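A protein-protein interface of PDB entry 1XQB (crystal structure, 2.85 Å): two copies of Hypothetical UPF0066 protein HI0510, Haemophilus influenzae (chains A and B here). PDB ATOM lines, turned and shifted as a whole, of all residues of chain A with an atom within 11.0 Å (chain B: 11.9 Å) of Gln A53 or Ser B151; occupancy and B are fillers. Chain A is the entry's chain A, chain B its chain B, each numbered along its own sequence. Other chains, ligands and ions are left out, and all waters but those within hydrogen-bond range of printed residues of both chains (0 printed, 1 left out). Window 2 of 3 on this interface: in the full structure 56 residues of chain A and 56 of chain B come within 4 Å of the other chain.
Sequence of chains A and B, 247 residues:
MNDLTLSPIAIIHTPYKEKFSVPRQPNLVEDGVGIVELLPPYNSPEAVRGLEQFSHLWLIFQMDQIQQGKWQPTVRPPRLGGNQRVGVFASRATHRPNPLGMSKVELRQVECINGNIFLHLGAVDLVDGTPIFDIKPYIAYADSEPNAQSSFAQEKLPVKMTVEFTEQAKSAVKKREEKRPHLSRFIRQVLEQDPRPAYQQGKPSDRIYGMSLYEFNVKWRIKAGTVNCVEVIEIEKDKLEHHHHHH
O of Ala A47 lies close to N of Phe B89 (3.5 Å).
The backbone carbonyl oxygen (O) of Arg A49 lies within hydrogen-bond range of the backbone NH (N) of Gly B87 (3.1 Å).
The side-chain hydroxyl (OG) of Ser A55 is in hydrogen-bond range of the backbone NH (N) of Gln B149 (3.3 Å).
O of Ser B150 lies close to O of Gln A53.
The backbone NH (N) of Tyr A138 lies within hydrogen-bond range of the backbone carbonyl oxygen (O) of His A56, 2.9 Å away.
OE2 of Glu A52 lies close to OE1 of Gln A53.
OG of Ser B91 is in hydrogen-bond range of O of Val B88, at 3.1 Å.
N of Leu A107 is in hydrogen-bond range of O of Ser A55 (2.8 Å).
Ala A47 touches Gly B87 (O to CA, 3.8 Å).
Ala A47 touches Val B88 (O to N, 3.7 Å).
Arg A49 touches Val B86.
Leu A51 touches Ala B90.
Gln A53 touches Ser B151.
Phe A54 touches Ala B90 (CE1 to O, 3.1 Å).
O of Phe B89 touches CG of Pro A137 (3.6 Å).
Ala B90 touches Pro A137 (O to CG, 3.3 Å).
Tyr A138 touches Ala B148 (CD2 to CB, 3.6 Å).
CB of Ala B148 touches CB of Ala A140, 3.8 Å away.
Of the printed residues of chain B, Gln A53 touches Ser B150 and Ser B151.
Ser B151 touches just one residue of chain A: Gln A53 (3.3 Å).
Of chain B, only Phe B89 (3.8 Å) and Ala B90 (3.9 Å) come within 4 Å of Leu A51.
No residue of chain B comes within 4 Å of Glu A52.
Of chain A, only Gln A53 (2.6 Å) comes within 4 Å of Ser B150.
Of the printed residues of chain B, Tyr A138 touches Ala B148.
Of the printed residues of chain B, Lys A136 touches Phe B89 (3.9 Å) and Arg B92 (3.98 Å).
Of the printed residues of chain B, Arg A49 touches Val B86, Gly B87 and Ala B90.
Of the printed residues of chain A, Ser B91 touches Pro A137 (3.2 Å).
Printed residues of chain B within 4 Å of Ser A55: Ala B148 and Gln B149.
The nearest residue of chain A that does not touch Ser B151 is Phe A54 (5.5 Å).
Printed residues of chain B that touch a printed residue of chain A: Val B86, Gly B87, Val B88, Phe B89, Ala B90, Ser B91, Arg B92, Ala B148, Gln B149, Ser B150 and Ser B151.
Of the 24 printed residues of chain A, 10 touch a printed residue of chain B.
Hydrophobic or aromatic side chains of chain A within 4 Å of the printed part of chain B: Ala A47, Leu A51, Phe A54, Pro A137, Tyr A138 and Ala A140.
No position is printed for both chains.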
ATOM      1  N   ALA A  47      -6.791 -25.675  -9.746  1.00  0.00           N
ATOM      2  CA  ALA A  47      -6.604 -24.234  -9.542  1.00  0.00           C
ATOM      3  C   ALA A  47      -7.092 -23.332 -10.689  1.00  0.00           C
ATOM      4  O   ALA A  47      -7.237 -22.124 -10.504  1.00  0.00           O
ATOM      5  CB  ALA A  47      -5.146 -23.941  -9.241  1.00  0.00           C
ATOM      6  N   VAL A  48      -7.310 -23.902 -11.872  1.00  0.00           N
ATOM      7  CA  VAL A  48      -7.779 -23.123 -13.014  1.00  0.00           C
ATOM      8  C   VAL A  48      -9.083 -23.669 -13.589  1.00  0.00           C
ATOM      9  O   VAL A  48      -9.497 -23.266 -14.680  1.00  0.00           O
ATOM     10  CB  VAL A  48      -6.731 -23.082 -14.160  1.00  0.00           C
ATOM     11  CG1 VAL A  48      -5.459 -22.380 -13.696  1.00  0.00           C
ATOM     12  CG2 VAL A  48      -6.434 -24.490 -14.659  1.00  0.00           C
ATOM     13  N   ARG A  49      -9.729 -24.580 -12.857  1.00  0.00           N
ATOM     14  CA  ARG A  49     -10.983 -25.193 -13.312  1.00  0.00           C
ATOM     15  C   ARG A  49     -12.062 -24.173 -13.642  1.00  0.00           C
ATOM     16  O   ARG A  49     -12.554 -23.464 -12.772  1.00  0.00           O
ATOM     17  CB  ARG A  49     -11.503 -26.208 -12.283  1.00  0.00           C
ATOM     18  CG  ARG A  49     -12.851 -26.846 -12.654  1.00  0.00           C
ATOM     19  CD  ARG A  49     -13.256 -27.963 -11.683  1.00  0.00           C
ATOM     20  NE  ARG A  49     -12.455 -29.169 -11.893  1.00  0.00           N
ATOM     21  CZ  ARG A  49     -11.812 -29.835 -10.937  1.00  0.00           C
ATOM     22  NH1 ARG A  49     -11.871 -29.431  -9.674  1.00  0.00           N
ATOM     23  NH2 ARG A  49     -11.061 -30.880 -11.259  1.00  0.00           N
ATOM     24  N   GLY A  50     -12.411 -24.103 -14.918  1.00  0.00           N
ATOM     25  CA  GLY A  50     -13.429 -23.169 -15.347  1.00  0.00           C
ATOM     26  C   GLY A  50     -12.910 -21.783 -15.679  1.00  0.00           C
ATOM     27  O   GLY A  50     -13.697 -20.885 -15.939  1.00  0.00           O
ATOM     28  N   LEU A  51     -11.593 -21.596 -15.691  1.00  0.00           N
ATOM     29  CA  LEU A  51     -11.020 -20.285 -15.996  1.00  0.00           C
ATOM     30  C   LEU A  51     -11.404 -19.915 -17.424  1.00  0.00           C
ATOM     31  O   LEU A  51     -11.647 -18.747 -17.739  1.00  0.00           O
ATOM     32  CB  LEU A  51      -9.496 -20.330 -15.875  1.00  0.00           C
ATOM     33  CG  LEU A  51      -8.713 -19.242 -15.141  1.00  0.00           C
ATOM     34  CD1 LEU A  51      -7.332 -19.156 -15.750  1.00  0.00           C
ATOM     35  CD2 LEU A  51      -9.403 -17.921 -15.242  1.00  0.00           C
ATOM     36  N   GLU A  52     -11.488 -20.935 -18.276  1.00  0.00           N
ATOM     37  CA  GLU A  52     -11.844 -20.755 -19.680  1.00  0.00           C
ATOM     38  C   GLU A  52     -13.240 -20.172 -19.879  1.00  0.00           C
ATOM     39  O   GLU A  52     -13.625 -19.847 -21.003  1.00  0.00           O
ATOM     40  CB  GLU A  52     -11.709 -22.078 -20.446  1.00  0.00           C
ATOM     41  CG  GLU A  52     -11.477 -23.321 -19.575  1.00  0.00           C
ATOM     42  CD  GLU A  52     -12.711 -23.774 -18.795  1.00  0.00           C
ATOM     43  OE1 GLU A  52     -12.559 -24.642 -17.903  1.00  0.00           O
ATOM     44  OE2 GLU A  52     -13.829 -23.284 -19.075  1.00  0.00           O
ATOM     45  N   GLN A  53     -13.989 -20.048 -18.784  1.00  0.00           N
ATOM     46  CA  GLN A  53     -15.339 -19.489 -18.818  1.00  0.00           C
ATOM     47  C   GLN A  53     -15.275 -18.019 -19.190  1.00  0.00           C
ATOM     48  O   GLN A  53     -15.923 -17.583 -20.136  1.00  0.00           O
ATOM     49  CB  GLN A  53     -16.021 -19.605 -17.446  1.00  0.00           C
ATOM     50  CG  GLN A  53     -16.387 -21.015 -16.995  1.00  0.00           C
ATOM     51  CD  GLN A  53     -17.387 -21.691 -17.911  1.00  0.00           C
ATOM     52  OE1 GLN A  53     -17.011 -22.265 -18.941  1.00  0.00           O
ATOM     53  NE2 GLN A  53     -18.671 -21.629 -17.544  1.00  0.00           N
ATOM     54  N   PHE A  54     -14.482 -17.268 -18.430  1.00  0.00           N
ATOM     55  CA  PHE A  54     -14.332 -15.834 -18.635  1.00  0.00           C
ATOM     56  C   PHE A  54     -13.432 -15.534 -19.821  1.00  0.00           C
ATOM     57  O   PHE A  54     -12.574 -16.337 -20.170  1.00  0.00           O
ATOM     58  CB  PHE A  54     -13.798 -15.180 -17.360  1.00  0.00           C
ATOM     59  CG  PHE A  54     -14.597 -15.524 -16.124  1.00  0.00           C
ATOM     60  CD1 PHE A  54     -14.253 -16.617 -15.340  1.00  0.00           C
ATOM     61  CD2 PHE A  54     -15.695 -14.759 -15.746  1.00  0.00           C
ATOM     62  CE1 PHE A  54     -14.987 -16.942 -14.204  1.00  0.00           C
ATOM     63  CE2 PHE A  54     -16.439 -15.082 -14.605  1.00  0.00           C
ATOM     64  CZ  PHE A  54     -16.081 -16.174 -13.837  1.00  0.00           C
ATOM     65  N   SER A  55     -13.671 -14.402 -20.471  1.00  0.00           N
ATOM     66  CA  SER A  55     -12.883 -14.020 -21.634  1.00  0.00           C
ATOM     67  C   SER A  55     -11.724 -13.123 -21.262  1.00  0.00           C
ATOM     68  O   SER A  55     -10.757 -13.008 -22.010  1.00  0.00           O
ATOM     69  CB  SER A  55     -13.746 -13.280 -22.656  1.00  0.00           C
ATOM     70  OG  SER A  55     -14.129 -12.006 -22.172  1.00  0.00           O
ATOM     71  N   HIS A  56     -11.849 -12.435 -20.136  1.00  0.00           N
ATOM     72  CA  HIS A  56     -10.805 -11.528 -19.714  1.00  0.00           C
ATOM     73  C   HIS A  56     -10.303 -11.834 -18.321  1.00  0.00           C
ATOM     74  O   HIS A  56     -11.030 -12.362 -17.495  1.00  0.00           O
ATOM     75  CB  HIS A  56     -11.283 -10.082 -19.841  1.00  0.00           C
ATOM     76  CG  HIS A  56     -11.365  -9.601 -21.255  1.00  0.00           C
ATOM     77  ND1 HIS A  56     -10.263  -9.155 -21.951  1.00  0.00           N
ATOM     78  CD2 HIS A  56     -12.407  -9.523 -22.112  1.00  0.00           C
ATOM     79  CE1 HIS A  56     -10.622  -8.828 -23.179  1.00  0.00           C
ATOM     80  NE2 HIS A  56     -11.919  -9.041 -23.302  1.00  0.00           N
ATOM     81  N   LEU A  57      -9.046 -11.500 -18.069  1.00  0.00           N
ATOM     82  CA  LEU A  57      -8.430 -11.774 -16.787  1.00  0.00           C
ATOM     83  C   LEU A  57      -7.683 -10.567 -16.186  1.00  0.00           C
ATOM     84  O   LEU A  57      -7.402  -9.589 -16.877  1.00  0.00           O
ATOM     85  CB  LEU A  57      -7.446 -12.943 -16.968  1.00  0.00           C
ATOM     86  CG  LEU A  57      -7.762 -14.393 -16.579  1.00  0.00           C
ATOM     87  CD1 LEU A  57      -9.160 -14.814 -17.020  1.00  0.00           C
ATOM     88  CD2 LEU A  57      -6.703 -15.301 -17.197  1.00  0.00           C
ATOM     89  N   VAL A 105      -5.782  -8.642 -19.299  1.00  0.00           N
ATOM     90  CA  VAL A 105      -5.437  -9.255 -20.572  1.00  0.00           C
ATOM     91  C   VAL A 105      -6.558 -10.159 -21.063  1.00  0.00           C
ATOM     92  O   VAL A 105      -7.436 -10.550 -20.289  1.00  0.00           O
ATOM     93  CB  VAL A 105      -4.128 -10.069 -20.441  1.00  0.00           C
ATOM     94  CG1 VAL A 105      -2.988  -9.158 -20.027  1.00  0.00           C
ATOM     95  CG2 VAL A 105      -4.288 -11.172 -19.398  1.00  0.00           C
ATOM     96  N   GLU A 106      -6.536 -10.467 -22.356  1.00  0.00           N
ATOM     97  CA  GLU A 106      -7.541 -11.334 -22.977  1.00  0.00           C
ATOM     98  C   GLU A 106      -7.135 -12.809 -22.817  1.00  0.00           C
ATOM     99  O   GLU A 106      -5.972 -13.171 -23.015  1.00  0.00           O
ATOM    100  CB  GLU A 106      -7.700 -10.951 -24.463  1.00  0.00           C
ATOM    101  CG  GLU A 106      -8.389 -11.979 -25.379  1.00  0.00           C
ATOM    102  CD  GLU A 106      -9.909 -12.072 -25.196  1.00  0.00           C
ATOM    103  OE1 GLU A 106     -10.409 -13.178 -24.870  1.00  0.00           O
ATOM    104  OE2 GLU A 106     -10.605 -11.052 -25.409  1.00  0.00           O
ATOM    105  N   LEU A 107      -8.078 -13.645 -22.395  1.00  0.00           N
ATOM    106  CA  LEU A 107      -7.793 -15.063 -22.219  1.00  0.00           C
ATOM    107  C   LEU A 107      -8.212 -15.853 -23.448  1.00  0.00           C
ATOM    108  O   LEU A 107      -9.403 -16.033 -23.707  1.00  0.00           O
ATOM    109  CB  LEU A 107      -8.487 -15.627 -20.973  1.00  0.00           C
ATOM    110  CG  LEU A 107      -8.315 -17.137 -20.744  1.00  0.00           C
ATOM    111  CD1 LEU A 107      -6.852 -17.548 -20.863  1.00  0.00           C
ATOM    112  CD2 LEU A 107      -8.867 -17.520 -19.376  1.00  0.00           C
ATOM    113  N   ARG A 108      -7.217 -16.361 -24.166  1.00  0.00           N
ATOM    114  CA  ARG A 108      -7.455 -17.130 -25.372  1.00  0.00           C
ATOM    115  C   ARG A 108      -7.503 -18.638 -25.185  1.00  0.00           C
ATOM    116  O   ARG A 108      -8.273 -19.325 -25.860  1.00  0.00           O
ATOM    117  CB  ARG A 108      -6.409 -16.781 -26.429  1.00  0.00           C
ATOM    118  CG  ARG A 108      -6.582 -15.402 -27.033  1.00  0.00           C
ATOM    119  CD  ARG A 108      -5.639 -15.213 -28.200  1.00  0.00           C
ATOM    120  NE  ARG A 108      -5.678 -13.848 -28.715  1.00  0.00           N
ATOM    121  CZ  ARG A 108      -4.764 -13.327 -29.528  1.00  0.00           C
ATOM    122  NH1 ARG A 108      -3.731 -14.063 -29.930  1.00  0.00           N
ATOM    123  NH2 ARG A 108      -4.864 -12.055 -29.903  1.00  0.00           N
ATOM    124  N   GLN A 109      -6.713 -19.152 -24.251  1.00  0.00           N
ATOM    125  CA  GLN A 109      -6.673 -20.594 -24.043  1.00  0.00           C
ATOM    126  C   GLN A 109      -5.985 -21.029 -22.761  1.00  0.00           C
ATOM    127  O   GLN A 109      -4.856 -20.639 -22.496  1.00  0.00           O
ATOM    128  CB  GLN A 109      -5.958 -21.243 -25.243  1.00  0.00           C
ATOM    129  CG  GLN A 109      -5.473 -22.674 -25.038  1.00  0.00           C
ATOM    130  CD  GLN A 109      -4.333 -23.053 -25.980  1.00  0.00           C
ATOM    131  OE1 GLN A 109      -4.115 -24.230 -26.262  1.00  0.00           O
ATOM    132  NE2 GLN A 109      -3.599 -22.054 -26.465  1.00  0.00           N
ATOM    133  N   VAL A 110      -6.675 -21.840 -21.969  1.00  0.00           N
ATOM    134  CA  VAL A 110      -6.095 -22.383 -20.743  1.00  0.00           C
ATOM    135  C   VAL A 110      -5.585 -23.777 -21.145  1.00  0.00           C
ATOM    136  O   VAL A 110      -6.381 -24.688 -21.369  1.00  0.00           O
ATOM    137  CB  VAL A 110      -7.146 -22.504 -19.609  1.00  0.00           C
ATOM    138  CG1 VAL A 110      -6.510 -23.088 -18.350  1.00  0.00           C
ATOM    139  CG2 VAL A 110      -7.746 -21.145 -19.308  1.00  0.00           C
ATOM    140  N   GLU A 111      -4.265 -23.927 -21.263  1.00  0.00           N
ATOM    141  CA  GLU A 111      -3.656 -25.189 -21.681  1.00  0.00           C
ATOM    142  C   GLU A 111      -3.028 -26.013 -20.558  1.00  0.00           C
ATOM    143  O   GLU A 111      -2.159 -25.526 -19.835  1.00  0.00           O
ATOM    144  CB  GLU A 111      -2.603 -24.907 -22.762  1.00  0.00           C
ATOM    145  CG  GLU A 111      -1.876 -26.127 -23.313  1.00  0.00           C
ATOM    146  CD  GLU A 111      -0.664 -25.763 -24.178  1.00  0.00           C
ATOM    147  OE1 GLU A 111       0.368 -25.318 -23.626  1.00  0.00           O
ATOM    148  OE2 GLU A 111      -0.738 -25.944 -25.415  1.00  0.00           O
ATOM    149  N   LEU A 119      -1.539 -20.256 -19.570  1.00  0.00           N
ATOM    150  CA  LEU A 119      -2.694 -19.415 -19.858  1.00  0.00           C
ATOM    151  C   LEU A 119      -2.242 -18.599 -21.057  1.00  0.00           C
ATOM    152  O   LEU A 119      -1.398 -17.701 -20.920  1.00  0.00           O
ATOM    153  CB  LEU A 119      -3.005 -18.472 -18.693  1.00  0.00           C
ATOM    154  CG  LEU A 119      -3.163 -19.119 -17.323  1.00  0.00           C
ATOM    155  CD1 LEU A 119      -3.561 -18.059 -16.315  1.00  0.00           C
ATOM    156  CD2 LEU A 119      -4.202 -20.220 -17.374  1.00  0.00           C
ATOM    157  N   LYS A 136      -6.994 -13.249 -11.425  1.00  0.00           N
ATOM    158  CA  LYS A 136      -8.423 -13.114 -11.164  1.00  0.00           C
ATOM    159  C   LYS A 136      -9.175 -12.984 -12.467  1.00  0.00           C
ATOM    160  O   LYS A 136      -8.587 -12.618 -13.484  1.00  0.00           O
ATOM    161  CB  LYS A 136      -8.702 -11.853 -10.354  1.00  0.00           C
ATOM    162  CG  LYS A 136      -8.105 -11.837  -8.981  1.00  0.00           C
ATOM    163  CD  LYS A 136      -8.644 -10.667  -8.181  1.00  0.00           C
ATOM    164  CE  LYS A 136      -7.996 -10.612  -6.793  1.00  0.00           C
ATOM    165  NZ  LYS A 136      -8.275 -11.803  -5.933  1.00  0.00           N
ATOM    166  N   PRO A 137     -10.492 -13.285 -12.464  1.00  0.00           N
ATOM    167  CA  PRO A 137     -11.285 -13.164 -13.694  1.00  0.00           C
ATOM    168  C   PRO A 137     -11.765 -11.718 -13.754  1.00  0.00           C
ATOM    169  O   PRO A 137     -12.162 -11.154 -12.722  1.00  0.00           O
ATOM    170  CB  PRO A 137     -12.486 -14.074 -13.436  1.00  0.00           C
ATOM    171  CG  PRO A 137     -12.224 -14.714 -12.112  1.00  0.00           C
ATOM    172  CD  PRO A 137     -11.338 -13.782 -11.375  1.00  0.00           C
ATOM    173  N   TYR A 138     -11.709 -11.103 -14.932  1.00  0.00           N
ATOM    174  CA  TYR A 138     -12.182  -9.731 -15.077  1.00  0.00           C
ATOM    175  C   TYR A 138     -13.688  -9.766 -15.215  1.00  0.00           C
ATOM    176  O   TYR A 138     -14.201 -10.305 -16.185  1.00  0.00           O
ATOM    177  CB  TYR A 138     -11.559  -9.077 -16.309  1.00  0.00           C
ATOM    178  CG  TYR A 138     -12.016  -7.655 -16.557  1.00  0.00           C
ATOM    179  CD1 TYR A 138     -11.157  -6.578 -16.335  1.00  0.00           C
ATOM    180  CD2 TYR A 138     -13.309  -7.386 -17.005  1.00  0.00           C
ATOM    181  CE1 TYR A 138     -11.581  -5.269 -16.555  1.00  0.00           C
ATOM    182  CE2 TYR A 138     -13.744  -6.098 -17.218  1.00  0.00           C
ATOM    183  CZ  TYR A 138     -12.884  -5.038 -16.995  1.00  0.00           C
ATOM    184  OH  TYR A 138     -13.335  -3.750 -17.209  1.00  0.00           O
ATOM    185  N   ILE A 139     -14.391  -9.230 -14.222  1.00  0.00           N
ATOM    186  CA  ILE A 139     -15.853  -9.182 -14.243  1.00  0.00           C
ATOM    187  C   ILE A 139     -16.300  -7.765 -14.598  1.00  0.00           C
ATOM    188  O   ILE A 139     -15.965  -6.805 -13.897  1.00  0.00           O
ATOM    189  CB  ILE A 139     -16.474  -9.605 -12.887  1.00  0.00           C
ATOM    190  CG1 ILE A 139     -15.968 -10.992 -12.475  1.00  0.00           C
ATOM    191  CG2 ILE A 139     -17.994  -9.635 -12.995  1.00  0.00           C
ATOM    192  CD1 ILE A 139     -16.475 -11.450 -11.134  1.00  0.00           C
ATOM    193  N   ALA A 140     -17.063  -7.651 -15.687  1.00  0.00           N
ATOM    194  CA  ALA A 140     -17.557  -6.368 -16.198  1.00  0.00           C
ATOM    195  C   ALA A 140     -18.397  -5.546 -15.226  1.00  0.00           C
ATOM    196  O   ALA A 140     -18.392  -4.314 -15.280  1.00  0.00           O
ATOM    197  CB  ALA A 140     -18.319  -6.583 -17.496  1.00  0.00           C
ATOM    198  N   VAL B  86     -15.307 -24.502  -8.511  1.00  0.00           N
ATOM    199  CA  VAL B  86     -14.363 -23.944  -9.478  1.00  0.00           C
ATOM    200  C   VAL B  86     -12.996 -23.614  -8.868  1.00  0.00           C
ATOM    201  O   VAL B  86     -12.805 -23.681  -7.648  1.00  0.00           O
ATOM    202  CB  VAL B  86     -14.934 -22.678 -10.189  1.00  0.00           C
ATOM    203  CG1 VAL B  86     -16.006 -23.080 -11.198  1.00  0.00           C
ATOM    204  CG2 VAL B  86     -15.513 -21.707  -9.173  1.00  0.00           C
ATOM    205  N   GLY B  87     -12.045 -23.272  -9.734  1.00  0.00           N
ATOM    206  CA  GLY B  87     -10.703 -22.942  -9.286  1.00  0.00           C
ATOM    207  C   GLY B  87     -10.572 -21.583  -8.624  1.00  0.00           C
ATOM    208  O   GLY B  87     -11.354 -20.664  -8.893  1.00  0.00           O
ATOM    209  N   VAL B  88      -9.562 -21.455  -7.766  1.00  0.00           N
ATOM    210  CA  VAL B  88      -9.290 -20.212  -7.050  1.00  0.00           C
ATOM    211  C   VAL B  88      -9.215 -19.054  -8.039  1.00  0.00           C
ATOM    212  O   VAL B  88      -9.976 -18.099  -7.944  1.00  0.00           O
ATOM    213  CB  VAL B  88      -7.941 -20.259  -6.308  1.00  0.00           C
ATOM    214  CG1 VAL B  88      -7.942 -19.263  -5.178  1.00  0.00           C
ATOM    215  CG2 VAL B  88      -7.646 -21.653  -5.818  1.00  0.00           C
ATOM    216  N   PHE B  89      -8.331 -19.188  -9.024  1.00  0.00           N
ATOM    217  CA  PHE B  89      -8.122 -18.174 -10.047  1.00  0.00           C
ATOM    218  C   PHE B  89      -9.343 -17.891 -10.919  1.00  0.00           C
ATOM    219  O   PHE B  89      -9.423 -16.834 -11.554  1.00  0.00           O
ATOM    220  CB  PHE B  89      -6.932 -18.581 -10.897  1.00  0.00           C
ATOM    221  CG  PHE B  89      -5.700 -18.880 -10.089  1.00  0.00           C
ATOM    222  CD1 PHE B  89      -5.012 -20.065 -10.267  1.00  0.00           C
ATOM    223  CD2 PHE B  89      -5.211 -17.949  -9.167  1.00  0.00           C
ATOM    224  CE1 PHE B  89      -3.852 -20.322  -9.550  1.00  0.00           C
ATOM    225  CE2 PHE B  89      -4.057 -18.197  -8.448  1.00  0.00           C
ATOM    226  CZ  PHE B  89      -3.371 -19.383  -8.641  1.00  0.00           C
ATOM    227  N   ALA B  90     -10.301 -18.819 -10.922  1.00  0.00           N
ATOM    228  CA  ALA B  90     -11.535 -18.672 -11.700  1.00  0.00           C
ATOM    229  C   ALA B  90     -12.622 -17.889 -10.946  1.00  0.00           C
ATOM    230  O   ALA B  90     -13.672 -17.577 -11.509  1.00  0.00           O
ATOM    231  CB  ALA B  90     -12.064 -20.047 -12.115  1.00  0.00           C
ATOM    232  N   SER B  91     -12.355 -17.561  -9.684  1.00  0.00           N
ATOM    233  CA  SER B  91     -13.311 -16.826  -8.854  1.00  0.00           C
ATOM    234  C   SER B  91     -12.672 -15.609  -8.191  1.00  0.00           C
ATOM    235  O   SER B  91     -11.546 -15.238  -8.520  1.00  0.00           O
ATOM    236  CB  SER B  91     -13.874 -17.746  -7.762  1.00  0.00           C
ATOM    237  OG  SER B  91     -12.868 -18.091  -6.823  1.00  0.00           O
ATOM    238  N   ARG B  92     -13.406 -15.004  -7.254  1.00  0.00           N
ATOM    239  CA  ARG B  92     -12.956 -13.831  -6.501  1.00  0.00           C
ATOM    240  C   ARG B  92     -12.807 -14.168  -5.025  1.00  0.00           C
ATOM    241  O   ARG B  92     -12.806 -13.279  -4.176  1.00  0.00           O
ATOM    242  CB  ARG B  92     -13.960 -12.685  -6.649  1.00  0.00           C
ATOM    243  CG  ARG B  92     -13.793 -11.839  -7.901  1.00  0.00           C
ATOM    244  CD  ARG B  92     -12.603 -10.886  -7.800  1.00  0.00           C
ATOM    245  NE  ARG B  92     -12.584  -9.947  -8.925  1.00  0.00           N
ATOM    246  CZ  ARG B  92     -12.364  -8.640  -8.818  1.00  0.00           C
ATOM    247  NH1 ARG B  92     -12.130  -8.088  -7.628  1.00  0.00           N
ATOM    248  NH2 ARG B  92     -12.401  -7.880  -9.902  1.00  0.00           N
ATOM    249  N   ASN B 147     -17.796  -5.473 -22.512  1.00  0.00           N
ATOM    250  CA  ASN B 147     -18.330  -6.711 -23.090  1.00  0.00           C
ATOM    251  C   ASN B 147     -17.730  -8.000 -22.506  1.00  0.00           C
ATOM    252  O   ASN B 147     -17.994  -9.093 -23.015  1.00  0.00           O
ATOM    253  CB  ASN B 147     -18.179  -6.681 -24.620  1.00  0.00           C
ATOM    254  CG  ASN B 147     -18.632  -5.347 -25.230  1.00  0.00           C
ATOM    255  OD1 ASN B 147     -17.883  -4.361 -25.225  1.00  0.00           O
ATOM    256  ND2 ASN B 147     -19.861  -5.311 -25.743  1.00  0.00           N
ATOM    257  N   ALA B 148     -16.966  -7.865 -21.417  1.00  0.00           N
ATOM    258  CA  ALA B 148     -16.321  -8.991 -20.731  1.00  0.00           C
ATOM    259  C   ALA B 148     -17.315 -10.092 -20.414  1.00  0.00           C
ATOM    260  O   ALA B 148     -18.129  -9.953 -19.499  1.00  0.00           O
ATOM    261  CB  ALA B 148     -15.663  -8.516 -19.459  1.00  0.00           C
ATOM    262  N   GLN B 149     -17.208 -11.192 -21.161  1.00  0.00           N
ATOM    263  CA  GLN B 149     -18.087 -12.356 -21.034  1.00  0.00           C
ATOM    264  C   GLN B 149     -17.823 -13.359 -19.910  1.00  0.00           C
ATOM    265  O   GLN B 149     -16.827 -13.273 -19.198  1.00  0.00           O
ATOM    266  CB  GLN B 149     -18.158 -13.095 -22.373  1.00  0.00           C
ATOM    267  CG  GLN B 149     -19.220 -12.555 -23.314  1.00  0.00           C
ATOM    268  CD  GLN B 149     -20.614 -12.671 -22.723  1.00  0.00           C
ATOM    269  OE1 GLN B 149     -21.139 -11.715 -22.148  1.00  0.00           O
ATOM    270  NE2 GLN B 149     -21.210 -13.851 -22.844  1.00  0.00           N
ATOM    271  N   SER B 150     -18.731 -14.327 -19.787  1.00  0.00           N
ATOM    272  CA  SER B 150     -18.659 -15.371 -18.760  1.00  0.00           C
ATOM    273  C   SER B 150     -19.053 -16.748 -19.331  1.00  0.00           C
ATOM    274  O   SER B 150     -18.514 -17.183 -20.351  1.00  0.00           O
ATOM    275  CB  SER B 150     -19.591 -15.019 -17.585  1.00  0.00           C
ATOM    276  OG  SER B 150     -19.421 -13.679 -17.147  1.00  0.00           O
ATOM    277  N   SER B 151     -19.983 -17.425 -18.655  1.00  0.00           N
ATOM    278  CA  SER B 151     -20.475 -18.744 -19.066  1.00  0.00           C
ATOM    279  C   SER B 151     -21.443 -18.635 -20.244  1.00  0.00           C
ATOM    280  O   SER B 151     -21.408 -19.446 -21.168  1.00  0.00           O
ATOM    281  CB  SER B 151     -21.171 -19.448 -17.889  1.00  0.00           C
ATOM    282  OG  SER B 151     -22.320 -18.732 -17.450  1.00  0.00           O
